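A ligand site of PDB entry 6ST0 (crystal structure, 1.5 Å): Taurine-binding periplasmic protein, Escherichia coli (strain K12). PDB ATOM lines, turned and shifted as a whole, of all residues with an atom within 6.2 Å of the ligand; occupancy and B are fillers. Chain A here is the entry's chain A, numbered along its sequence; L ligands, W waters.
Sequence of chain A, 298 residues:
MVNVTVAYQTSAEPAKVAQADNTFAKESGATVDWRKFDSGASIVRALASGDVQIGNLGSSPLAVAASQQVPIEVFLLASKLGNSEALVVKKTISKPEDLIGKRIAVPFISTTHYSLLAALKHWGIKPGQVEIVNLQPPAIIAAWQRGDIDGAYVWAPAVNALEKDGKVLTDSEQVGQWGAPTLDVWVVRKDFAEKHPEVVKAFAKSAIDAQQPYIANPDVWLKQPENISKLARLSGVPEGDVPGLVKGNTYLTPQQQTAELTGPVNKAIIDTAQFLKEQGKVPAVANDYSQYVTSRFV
OD1 of Asn 56 is in hydrogen-bond range of N2 of the ligand. The backbone NH (N) of Thr 111 lies within hydrogen-bond range of an oxygen (O1) of the ligand (2.8 Å). OG1 of Thr 111 lies close to O1 of the ligand. OE2 of Glu 85 is in salt-bridge range of N1 of the ligand, at 2.8 Å. The side-chain amide nitrogen (NE2) of Gln 9 is in hydrogen-bond range of an oxygen (O2) of the ligand (2.9 Å). N of Gly 58 lies within hydrogen-bond range of O2 of the ligand, at 2.9 Å. N of Gly 40 lies within hydrogen-bond range of O3 of the ligand (2.9 Å). N1 of the ligand lies within salt-bridge range of OD1 of Asp 184, 3.0 Å away. The backbone NH of Ser 11 lies close to an oxygen (O4) of the ligand, 3.3 Å away.
N of Thr 10 touches O4 of the ligand, at 3.7 Å. Ser 39 touches the ligand. C of Leu 57 touches O2 of the ligand, at 3.9 Å. CD of Pro 61 touches O1 of the ligand, at 3.2 Å. Ser 110 touches the ligand. Trp 155 touches the ligand. Hydrophobic or aromatic side chains within 4 Å of the ligand: Pro 61 and Trp 155. 14 residues have an atom within 4 Å of the ligand: Gln 9, Thr 10, Ser 11, Ser 39, Gly 40, Asn 56, Leu 57, Gly 58, Pro 61, Glu 85, Ser 110, Thr 111, Trp 155 and Asp 184. The nearest printed residue that does not touch the ligand is Leu 81 (4.5 Å).
NE2 of Gln 9 lies within hydrogen-bond range of O of Asn 56 (2.8 Å). OG1 of Thr 111 lies within hydrogen-bond range of OE1 of Glu 85 (2.8 Å). The backbone carbonyl oxygen (O) of Gln 9 sits at hydrogen-bond distance from the side-chain amino group (NZ) of Lys 16 (2.8 Å). OG of Ser 110 lies within hydrogen-bond range of OG1 of Thr 112 (3.0 Å). The backbone carbonyl oxygen (O) of Pro 107 sits at hydrogen-bond distance from the side-chain hydroxyl (OG) of Ser 110 (2.7 Å). The side-chain amino group (NZ) of Lys 16 is in hydrogen-bond range of the backbone carbonyl oxygen (O) of Ser 11 (2.7 Å). OG1 of Thr 10 sits at hydrogen-bond distance from NE1 of Trp 155. The side-chain hydroxyl (OG1) of Thr 10 lies within hydrogen-bond range of the backbone carbonyl oxygen (O) of Ala 156 (2.6 Å).
Water W1 lies within hydrogen-bond range of an oxygen (O4) of the ligand (2.8 Å), the side-chain amino group (NZ) of Lys 16 (3.3 Å) and the backbone carbonyl oxygen (O) of Gln 9 (3.4 Å).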
ATOM      1  N   GLN A   9       2.829  32.585  -6.495  1.00  0.00           N
ATOM      2  CA  GLN A   9       1.887  31.830  -5.670  1.00  0.00           C
ATOM      3  C   GLN A   9       2.273  31.987  -4.200  1.00  0.00           C
ATOM      4  O   GLN A   9       3.231  32.699  -3.862  1.00  0.00           O
ATOM      5  CB  GLN A   9       1.860  30.357  -6.101  1.00  0.00           C
ATOM      6  CG  GLN A   9       1.268  30.146  -7.492  1.00  0.00           C
ATOM      7  CD  GLN A   9       0.751  28.728  -7.690  1.00  0.00           C
ATOM      8  OE1 GLN A   9      -0.120  28.276  -6.954  1.00  0.00           O
ATOM      9  NE2 GLN A   9       1.305  28.023  -8.685  1.00  0.00           N
ATOM     10  N   THR A  10       1.536  31.321  -3.307  1.00  0.00           N
ATOM     11  CA  THR A  10       1.510  31.723  -1.893  1.00  0.00           C
ATOM     12  C   THR A  10       2.322  30.822  -0.962  1.00  0.00           C
ATOM     13  O   THR A  10       2.237  30.992   0.253  1.00  0.00           O
ATOM     14  CB  THR A  10       0.078  31.808  -1.376  1.00  0.00           C
ATOM     15  OG1 THR A  10      -0.626  30.586  -1.645  1.00  0.00           O
ATOM     16  CG2 THR A  10      -0.664  32.969  -2.013  1.00  0.00           C
ATOM     17  N   SER A  11       3.119  29.894  -1.489  1.00  0.00           N
ATOM     18  CA  SER A  11       3.971  29.084  -0.623  1.00  0.00           C
ATOM     19  C   SER A  11       4.992  29.953   0.107  1.00  0.00           C
ATOM     20  O   SER A  11       5.584  30.874  -0.467  1.00  0.00           O
ATOM     21  CB  SER A  11       4.680  28.014  -1.454  1.00  0.00           C
ATOM     22  OG  SER A  11       5.664  27.320  -0.699  1.00  0.00           O
ATOM     23  N   ALA A  12       5.194  29.667   1.394  1.00  0.00           N
ATOM     24  CA  ALA A  12       6.183  30.381   2.197  1.00  0.00           C
ATOM     25  C   ALA A  12       7.529  29.690   2.021  1.00  0.00           C
ATOM     26  O   ALA A  12       7.755  28.606   2.561  1.00  0.00           O
ATOM     27  CB  ALA A  12       5.775  30.399   3.675  1.00  0.00           C
ATOM     28  N   LYS A  16      10.931  34.145  -1.260  1.00  0.00           N
ATOM     29  CA  LYS A  16      10.024  35.267  -1.038  1.00  0.00           C
ATOM     30  C   LYS A  16      10.742  36.471  -0.457  1.00  0.00           C
ATOM     31  O   LYS A  16      10.262  37.590  -0.614  1.00  0.00           O
ATOM     32  CB  LYS A  16       8.855  34.844  -0.137  1.00  0.00           C
ATOM     33  CG  LYS A  16       7.814  33.930  -0.799  1.00  0.00           C
ATOM     34  CD  LYS A  16       6.725  34.725  -1.506  1.00  0.00           C
ATOM     35  CE  LYS A  16       5.450  33.897  -1.729  1.00  0.00           C
ATOM     36  NZ  LYS A  16       5.669  32.625  -2.508  1.00  0.00           N
ATOM     37  N   ASP A  38      -4.013  32.228  -7.522  1.00  0.00           N
ATOM     38  CA  ASP A  38      -4.496  31.361  -6.455  1.00  0.00           C
ATOM     39  C   ASP A  38      -4.066  29.910  -6.634  1.00  0.00           C
ATOM     40  O   ASP A  38      -3.943  29.180  -5.644  1.00  0.00           O
ATOM     41  CB  ASP A  38      -6.020  31.462  -6.352  1.00  0.00           C
ATOM     42  CG  ASP A  38      -6.472  32.750  -5.694  1.00  0.00           C
ATOM     43  OD1 ASP A  38      -5.762  33.249  -4.796  1.00  0.00           O
ATOM     44  OD2 ASP A  38      -7.540  33.267  -6.087  1.00  0.00           O
ATOM     45  N   SER A  39      -3.852  29.486  -7.872  1.00  0.00           N
ATOM     46  CA  SER A  39      -3.300  28.164  -8.170  1.00  0.00           C
ATOM     47  C   SER A  39      -2.749  28.200  -9.598  1.00  0.00           C
ATOM     48  O   SER A  39      -2.840  29.209 -10.297  1.00  0.00           O
ATOM     49  CB  SER A  39      -4.342  27.061  -7.983  1.00  0.00           C
ATOM     50  OG  SER A  39      -5.436  27.226  -8.861  1.00  0.00           O
ATOM     51  N   GLY A  40      -2.186  27.067 -10.023  1.00  0.00           N
ATOM     52  CA  GLY A  40      -1.400  27.047 -11.254  1.00  0.00           C
ATOM     53  C   GLY A  40      -2.186  26.961 -12.542  1.00  0.00           C
ATOM     54  O   GLY A  40      -1.711  27.384 -13.589  1.00  0.00           O
ATOM     55  N   ALA A  41      -3.398  26.388 -12.503  1.00  0.00           N
ATOM     56  CA  ALA A  41      -4.157  26.249 -13.741  1.00  0.00           C
ATOM     57  C   ALA A  41      -4.367  27.602 -14.407  1.00  0.00           C
ATOM     58  O   ALA A  41      -4.198  27.733 -15.631  1.00  0.00           O
ATOM     59  CB  ALA A  41      -5.503  25.558 -13.477  1.00  0.00           C
ATOM     60  N   ILE A  43      -2.477  30.175 -14.073  1.00  0.00           N
ATOM     61  CA  ILE A  43      -1.182  30.646 -14.565  1.00  0.00           C
ATOM     62  C   ILE A  43      -0.880  30.052 -15.939  1.00  0.00           C
ATOM     63  O   ILE A  43      -0.333  30.739 -16.815  1.00  0.00           O
ATOM     64  CB  ILE A  43      -0.070  30.328 -13.558  1.00  0.00           C
ATOM     65  CG1 ILE A  43      -0.392  30.928 -12.191  1.00  0.00           C
ATOM     66  CG2 ILE A  43       1.298  30.856 -14.061  1.00  0.00           C
ATOM     67  CD1 ILE A  43       0.701  30.694 -11.160  1.00  0.00           C
ATOM     68  N   ASN A  56       5.289  30.777 -11.620  1.00  0.00           N
ATOM     69  CA  ASN A  56       5.563  29.679 -10.691  1.00  0.00           C
ATOM     70  C   ASN A  56       4.470  28.624 -10.827  1.00  0.00           C
ATOM     71  O   ASN A  56       3.302  28.888 -10.521  1.00  0.00           O
ATOM     72  CB  ASN A  56       5.641  30.220  -9.260  1.00  0.00           C
ATOM     73  CG  ASN A  56       6.021  29.171  -8.246  1.00  0.00           C
ATOM     74  OD1 ASN A  56       5.222  28.313  -7.892  1.00  0.00           O
ATOM     75  ND2 ASN A  56       7.248  29.237  -7.759  1.00  0.00           N
ATOM     76  N   LEU A  57       4.853  27.429 -11.259  1.00  0.00           N
ATOM     77  CA  LEU A  57       3.930  26.327 -11.504  1.00  0.00           C
ATOM     78  C   LEU A  57       4.282  25.117 -10.652  1.00  0.00           C
ATOM     79  O   LEU A  57       5.463  24.777 -10.502  1.00  0.00           O
ATOM     80  CB  LEU A  57       3.935  25.875 -12.984  1.00  0.00           C
ATOM     81  CG  LEU A  57       3.380  26.843 -14.019  1.00  0.00           C
ATOM     82  CD1 LEU A  57       3.402  26.212 -15.414  1.00  0.00           C
ATOM     83  CD2 LEU A  57       1.955  27.249 -13.630  1.00  0.00           C
ATOM     84  N   GLY A  58       3.256  24.464 -10.108  1.00  0.00           N
ATOM     85  CA  GLY A  58       3.450  23.114  -9.612  1.00  0.00           C
ATOM     86  C   GLY A  58       3.742  22.155 -10.753  1.00  0.00           C
ATOM     87  O   GLY A  58       3.474  22.432 -11.921  1.00  0.00           O
ATOM     88  N   SER A  59       4.316  21.003 -10.408  1.00  0.00           N
ATOM     89  CA  SER A  59       4.708  20.051 -11.448  1.00  0.00           C
ATOM     90  C   SER A  59       3.502  19.483 -12.182  1.00  0.00           C
ATOM     91  O   SER A  59       3.603  19.119 -13.367  1.00  0.00           O
ATOM     92  CB  SER A  59       5.560  18.940 -10.838  1.00  0.00           C
ATOM     93  OG  SER A  59       4.995  18.389  -9.665  1.00  0.00           O
ATOM     94  N   SER A  60       2.334  19.398 -11.529  1.00  0.00           N
ATOM     95  CA  SER A  60       1.141  18.903 -12.214  1.00  0.00           C
ATOM     96  C   SER A  60       0.605  19.906 -13.236  1.00  0.00           C
ATOM     97  O   SER A  60       0.353  19.506 -14.381  1.00  0.00           O
ATOM     98  CB  SER A  60       0.095  18.478 -11.177  1.00  0.00           C
ATOM     99  OG  SER A  60      -1.095  17.995 -11.789  1.00  0.00           O
ATOM    100  N   PRO A  61       0.421  21.192 -12.917  1.00  0.00           N
ATOM    101  CA  PRO A  61       0.060  22.130 -13.990  1.00  0.00           C
ATOM    102  C   PRO A  61       1.124  22.237 -15.075  1.00  0.00           C
ATOM    103  O   PRO A  61       0.797  22.435 -16.248  1.00  0.00           O
ATOM    104  CB  PRO A  61      -0.131  23.461 -13.237  1.00  0.00           C
ATOM    105  CG  PRO A  61      -0.572  23.027 -11.890  1.00  0.00           C
ATOM    106  CD  PRO A  61       0.274  21.818 -11.588  1.00  0.00           C
ATOM    107  N   LEU A  81       8.529  19.519  -2.964  1.00  0.00           N
ATOM    108  CA  LEU A  81       7.455  19.697  -2.000  1.00  0.00           C
ATOM    109  C   LEU A  81       7.428  18.575  -0.976  1.00  0.00           C
ATOM    110  O   LEU A  81       7.557  17.399  -1.333  1.00  0.00           O
ATOM    111  CB  LEU A  81       6.102  19.789  -2.713  1.00  0.00           C
ATOM    112  CG  LEU A  81       6.043  21.012  -3.631  1.00  0.00           C
ATOM    113  CD1 LEU A  81       4.795  20.973  -4.488  1.00  0.00           C
ATOM    114  CD2 LEU A  81       6.084  22.289  -2.782  1.00  0.00           C
ATOM    115  N   GLU A  85       2.494  20.922   1.869  1.00  0.00           N
ATOM    116  CA  GLU A  85       1.209  20.638   1.236  1.00  0.00           C
ATOM    117  C   GLU A  85       0.608  19.409   1.910  1.00  0.00           C
ATOM    118  O   GLU A  85       1.303  18.403   2.097  1.00  0.00           O
ATOM    119  CB  GLU A  85       1.393  20.417  -0.274  1.00  0.00           C
ATOM    120  CG  GLU A  85       2.245  21.504  -0.928  1.00  0.00           C
ATOM    121  CD  GLU A  85       1.909  21.767  -2.385  1.00  0.00           C
ATOM    122  OE1 GLU A  85       1.477  20.833  -3.095  1.00  0.00           O
ATOM    123  OE2 GLU A  85       2.095  22.933  -2.843  1.00  0.00           O
ATOM    124  N   PRO A 107      -7.764  22.479  -5.725  1.00  0.00           N
ATOM    125  CA  PRO A 107      -7.730  23.292  -6.947  1.00  0.00           C
ATOM    126  C   PRO A 107      -7.366  22.415  -8.135  1.00  0.00           C
ATOM    127  O   PRO A 107      -6.441  21.605  -8.061  1.00  0.00           O
ATOM    128  CB  PRO A 107      -6.653  24.354  -6.655  1.00  0.00           C
ATOM    129  CG  PRO A 107      -6.476  24.327  -5.144  1.00  0.00           C
ATOM    130  CD  PRO A 107      -6.739  22.897  -4.755  1.00  0.00           C
ATOM    131  N   PHE A 108      -8.122  22.578  -9.229  1.00  0.00           N
ATOM    132  CA  PHE A 108      -8.053  21.716 -10.408  1.00  0.00           C
ATOM    133  C   PHE A 108      -6.623  21.582 -10.932  1.00  0.00           C
ATOM    134  O   PHE A 108      -5.938  22.586 -11.160  1.00  0.00           O
ATOM    135  CB  PHE A 108      -8.955  22.305 -11.494  1.00  0.00           C
ATOM    136  CG  PHE A 108      -9.003  21.513 -12.782  1.00  0.00           C
ATOM    137  CD1 PHE A 108      -9.488  20.213 -12.805  1.00  0.00           C
ATOM    138  CD2 PHE A 108      -8.600  22.094 -13.981  1.00  0.00           C
ATOM    139  CE1 PHE A 108      -9.547  19.495 -13.999  1.00  0.00           C
ATOM    140  CE2 PHE A 108      -8.657  21.386 -15.174  1.00  0.00           C
ATOM    141  CZ  PHE A 108      -9.132  20.082 -15.189  1.00  0.00           C
ATOM    142  N   ILE A 109      -6.206  20.333 -11.142  1.00  0.00           N
ATOM    143  CA  ILE A 109      -4.918  19.846 -11.637  1.00  0.00           C
ATOM    144  C   ILE A 109      -3.712  20.492 -10.943  1.00  0.00           C
ATOM    145  O   ILE A 109      -2.576  20.412 -11.442  1.00  0.00           O
ATOM    146  CB  ILE A 109      -4.811  19.965 -13.171  1.00  0.00           C
ATOM    147  CG1 ILE A 109      -4.912  21.419 -13.673  1.00  0.00           C
ATOM    148  CG2 ILE A 109      -5.886  19.091 -13.843  1.00  0.00           C
ATOM    149  CD1 ILE A 109      -3.620  22.001 -14.139  1.00  0.00           C
ATOM    150  N   SER A 110      -3.913  21.063  -9.757  1.00  0.00           N
ATOM    151  CA  SER A 110      -2.804  21.488  -8.919  1.00  0.00           C
ATOM    152  C   SER A 110      -1.978  20.277  -8.473  1.00  0.00           C
ATOM    153  O   SER A 110      -2.350  19.116  -8.683  1.00  0.00           O
ATOM    154  CB  SER A 110      -3.320  22.250  -7.688  1.00  0.00           C
ATOM    155  OG  SER A 110      -4.055  21.384  -6.844  1.00  0.00           O
ATOM    156  N   THR A 111      -0.843  20.560  -7.811  1.00  0.00           N
ATOM    157  CA  THR A 111      -0.062  19.494  -7.185  1.00  0.00           C
ATOM    158  C   THR A 111      -0.851  18.749  -6.124  1.00  0.00           C
ATOM    159  O   THR A 111      -0.597  17.580  -5.885  1.00  0.00           O
ATOM    160  CB  THR A 111       1.190  20.052  -6.540  1.00  0.00           C
ATOM    161  OG1 THR A 111       0.853  21.219  -5.771  1.00  0.00           O
ATOM    162  CG2 THR A 111       2.243  20.385  -7.601  1.00  0.00           C
ATOM    163  N   THR A 112      -1.795  19.416  -5.453  1.00  0.00           N
ATOM    164  CA  THR A 112      -2.536  18.725  -4.421  1.00  0.00           C
ATOM    165  C   THR A 112      -3.716  17.943  -4.965  1.00  0.00           C
ATOM    166  O   THR A 112      -4.111  16.953  -4.354  1.00  0.00           O
ATOM    167  CB  THR A 112      -3.018  19.703  -3.335  1.00  0.00           C
ATOM    168  OG1 THR A 112      -3.867  20.707  -3.910  1.00  0.00           O
ATOM    169  CG2 THR A 112      -1.815  20.340  -2.652  1.00  0.00           C
ATOM    170  N   TRP A 155      -2.092  23.968   0.139  1.00  0.00           N
ATOM    171  CA  TRP A 155      -0.848  24.593   0.571  1.00  0.00           C
ATOM    172  C   TRP A 155      -1.194  25.890   1.299  1.00  0.00           C
ATOM    173  O   TRP A 155      -2.372  26.214   1.462  1.00  0.00           O
ATOM    174  CB  TRP A 155       0.090  24.823  -0.623  1.00  0.00           C
ATOM    175  CG  TRP A 155      -0.469  25.688  -1.742  1.00  0.00           C
ATOM    176  CD1 TRP A 155      -0.257  27.024  -1.934  1.00  0.00           C
ATOM    177  CD2 TRP A 155      -1.290  25.247  -2.832  1.00  0.00           C
ATOM    178  NE1 TRP A 155      -0.903  27.447  -3.076  1.00  0.00           N
ATOM    179  CE2 TRP A 155      -1.559  26.371  -3.636  1.00  0.00           C
ATOM    180  CE3 TRP A 155      -1.836  24.010  -3.195  1.00  0.00           C
ATOM    181  CZ2 TRP A 155      -2.351  26.301  -4.778  1.00  0.00           C
ATOM    182  CZ3 TRP A 155      -2.625  23.949  -4.336  1.00  0.00           C
ATOM    183  CH2 TRP A 155      -2.869  25.086  -5.121  1.00  0.00           C
ATOM    184  N   ALA A 156      -0.176  26.619   1.733  1.00  0.00           N
ATOM    185  CA  ALA A 156      -0.388  27.851   2.485  1.00  0.00           C
ATOM    186  C   ALA A 156      -1.009  28.930   1.607  1.00  0.00           C
ATOM    187  O   ALA A 156      -0.736  29.005   0.403  1.00  0.00           O
ATOM    188  CB  ALA A 156       0.926  28.350   3.074  1.00  0.00           C
ATOM    189  N   LEU A 183       6.762  18.954  -7.312  1.00  0.00           N
ATOM    190  CA  LEU A 183       7.715  20.063  -7.283  1.00  0.00           C
ATOM    191  C   LEU A 183       7.017  21.387  -7.526  1.00  0.00           C
ATOM    192  O   LEU A 183       5.942  21.433  -8.118  1.00  0.00           O
ATOM    193  CB  LEU A 183       8.801  19.926  -8.355  1.00  0.00           C
ATOM    194  CG  LEU A 183       9.517  18.635  -8.710  1.00  0.00           C
ATOM    195  CD1 LEU A 183      10.143  18.793 -10.089  1.00  0.00           C
ATOM    196  CD2 LEU A 183      10.590  18.353  -7.673  1.00  0.00           C
ATOM    197  N   ASP A 184       7.686  22.459  -7.141  1.00  0.00           N
ATOM    198  CA  ASP A 184       7.352  23.806  -7.600  1.00  0.00           C
ATOM    199  C   ASP A 184       8.487  24.297  -8.486  1.00  0.00           C
ATOM    200  O   ASP A 184       9.662  24.122  -8.139  1.00  0.00           O
ATOM    201  CB  ASP A 184       7.153  24.781  -6.418  1.00  0.00           C
ATOM    202  CG  ASP A 184       5.769  24.690  -5.820  1.00  0.00           C
ATOM    203  OD1 ASP A 184       4.818  24.351  -6.554  1.00  0.00           O
ATOM    204  OD2 ASP A 184       5.621  24.969  -4.622  1.00  0.00           O
HETATM  205  C1  LIG L   1       1.815  24.372  -6.480  1.00  0.00           C
HETATM  206  C2  LIG L   1       0.417  24.806  -6.752  1.00  0.00           C
HETATM  207  C3  LIG L   1       1.837  25.943  -4.549  1.00  0.00           C
HETATM  208  C4  LIG L   1       2.832  27.073  -4.879  1.00  0.00           C
HETATM  209  N1  LIG L   1       2.263  24.636  -5.084  1.00  0.00           N
HETATM  210  N2  LIG L   1       3.490  27.072  -6.101  1.00  0.00           N
HETATM  211  O1  LIG L   1       0.180  23.037  -8.593  1.00  0.00           O
HETATM  212  O2  LIG L   1       0.598  25.322  -9.287  1.00  0.00           O
HETATM  213  O3  LIG L   1      -1.540  24.718  -8.383  1.00  0.00           O
HETATM  214  O4  LIG L   1       3.084  28.016  -4.145  1.00  0.00           O
HETATM  215  S1  LIG L   1      -0.134  24.440  -8.405  1.00  0.00           S
HETATM  216  O   HOH W   1       5.137  29.952  -4.349  1.00  0.00           O
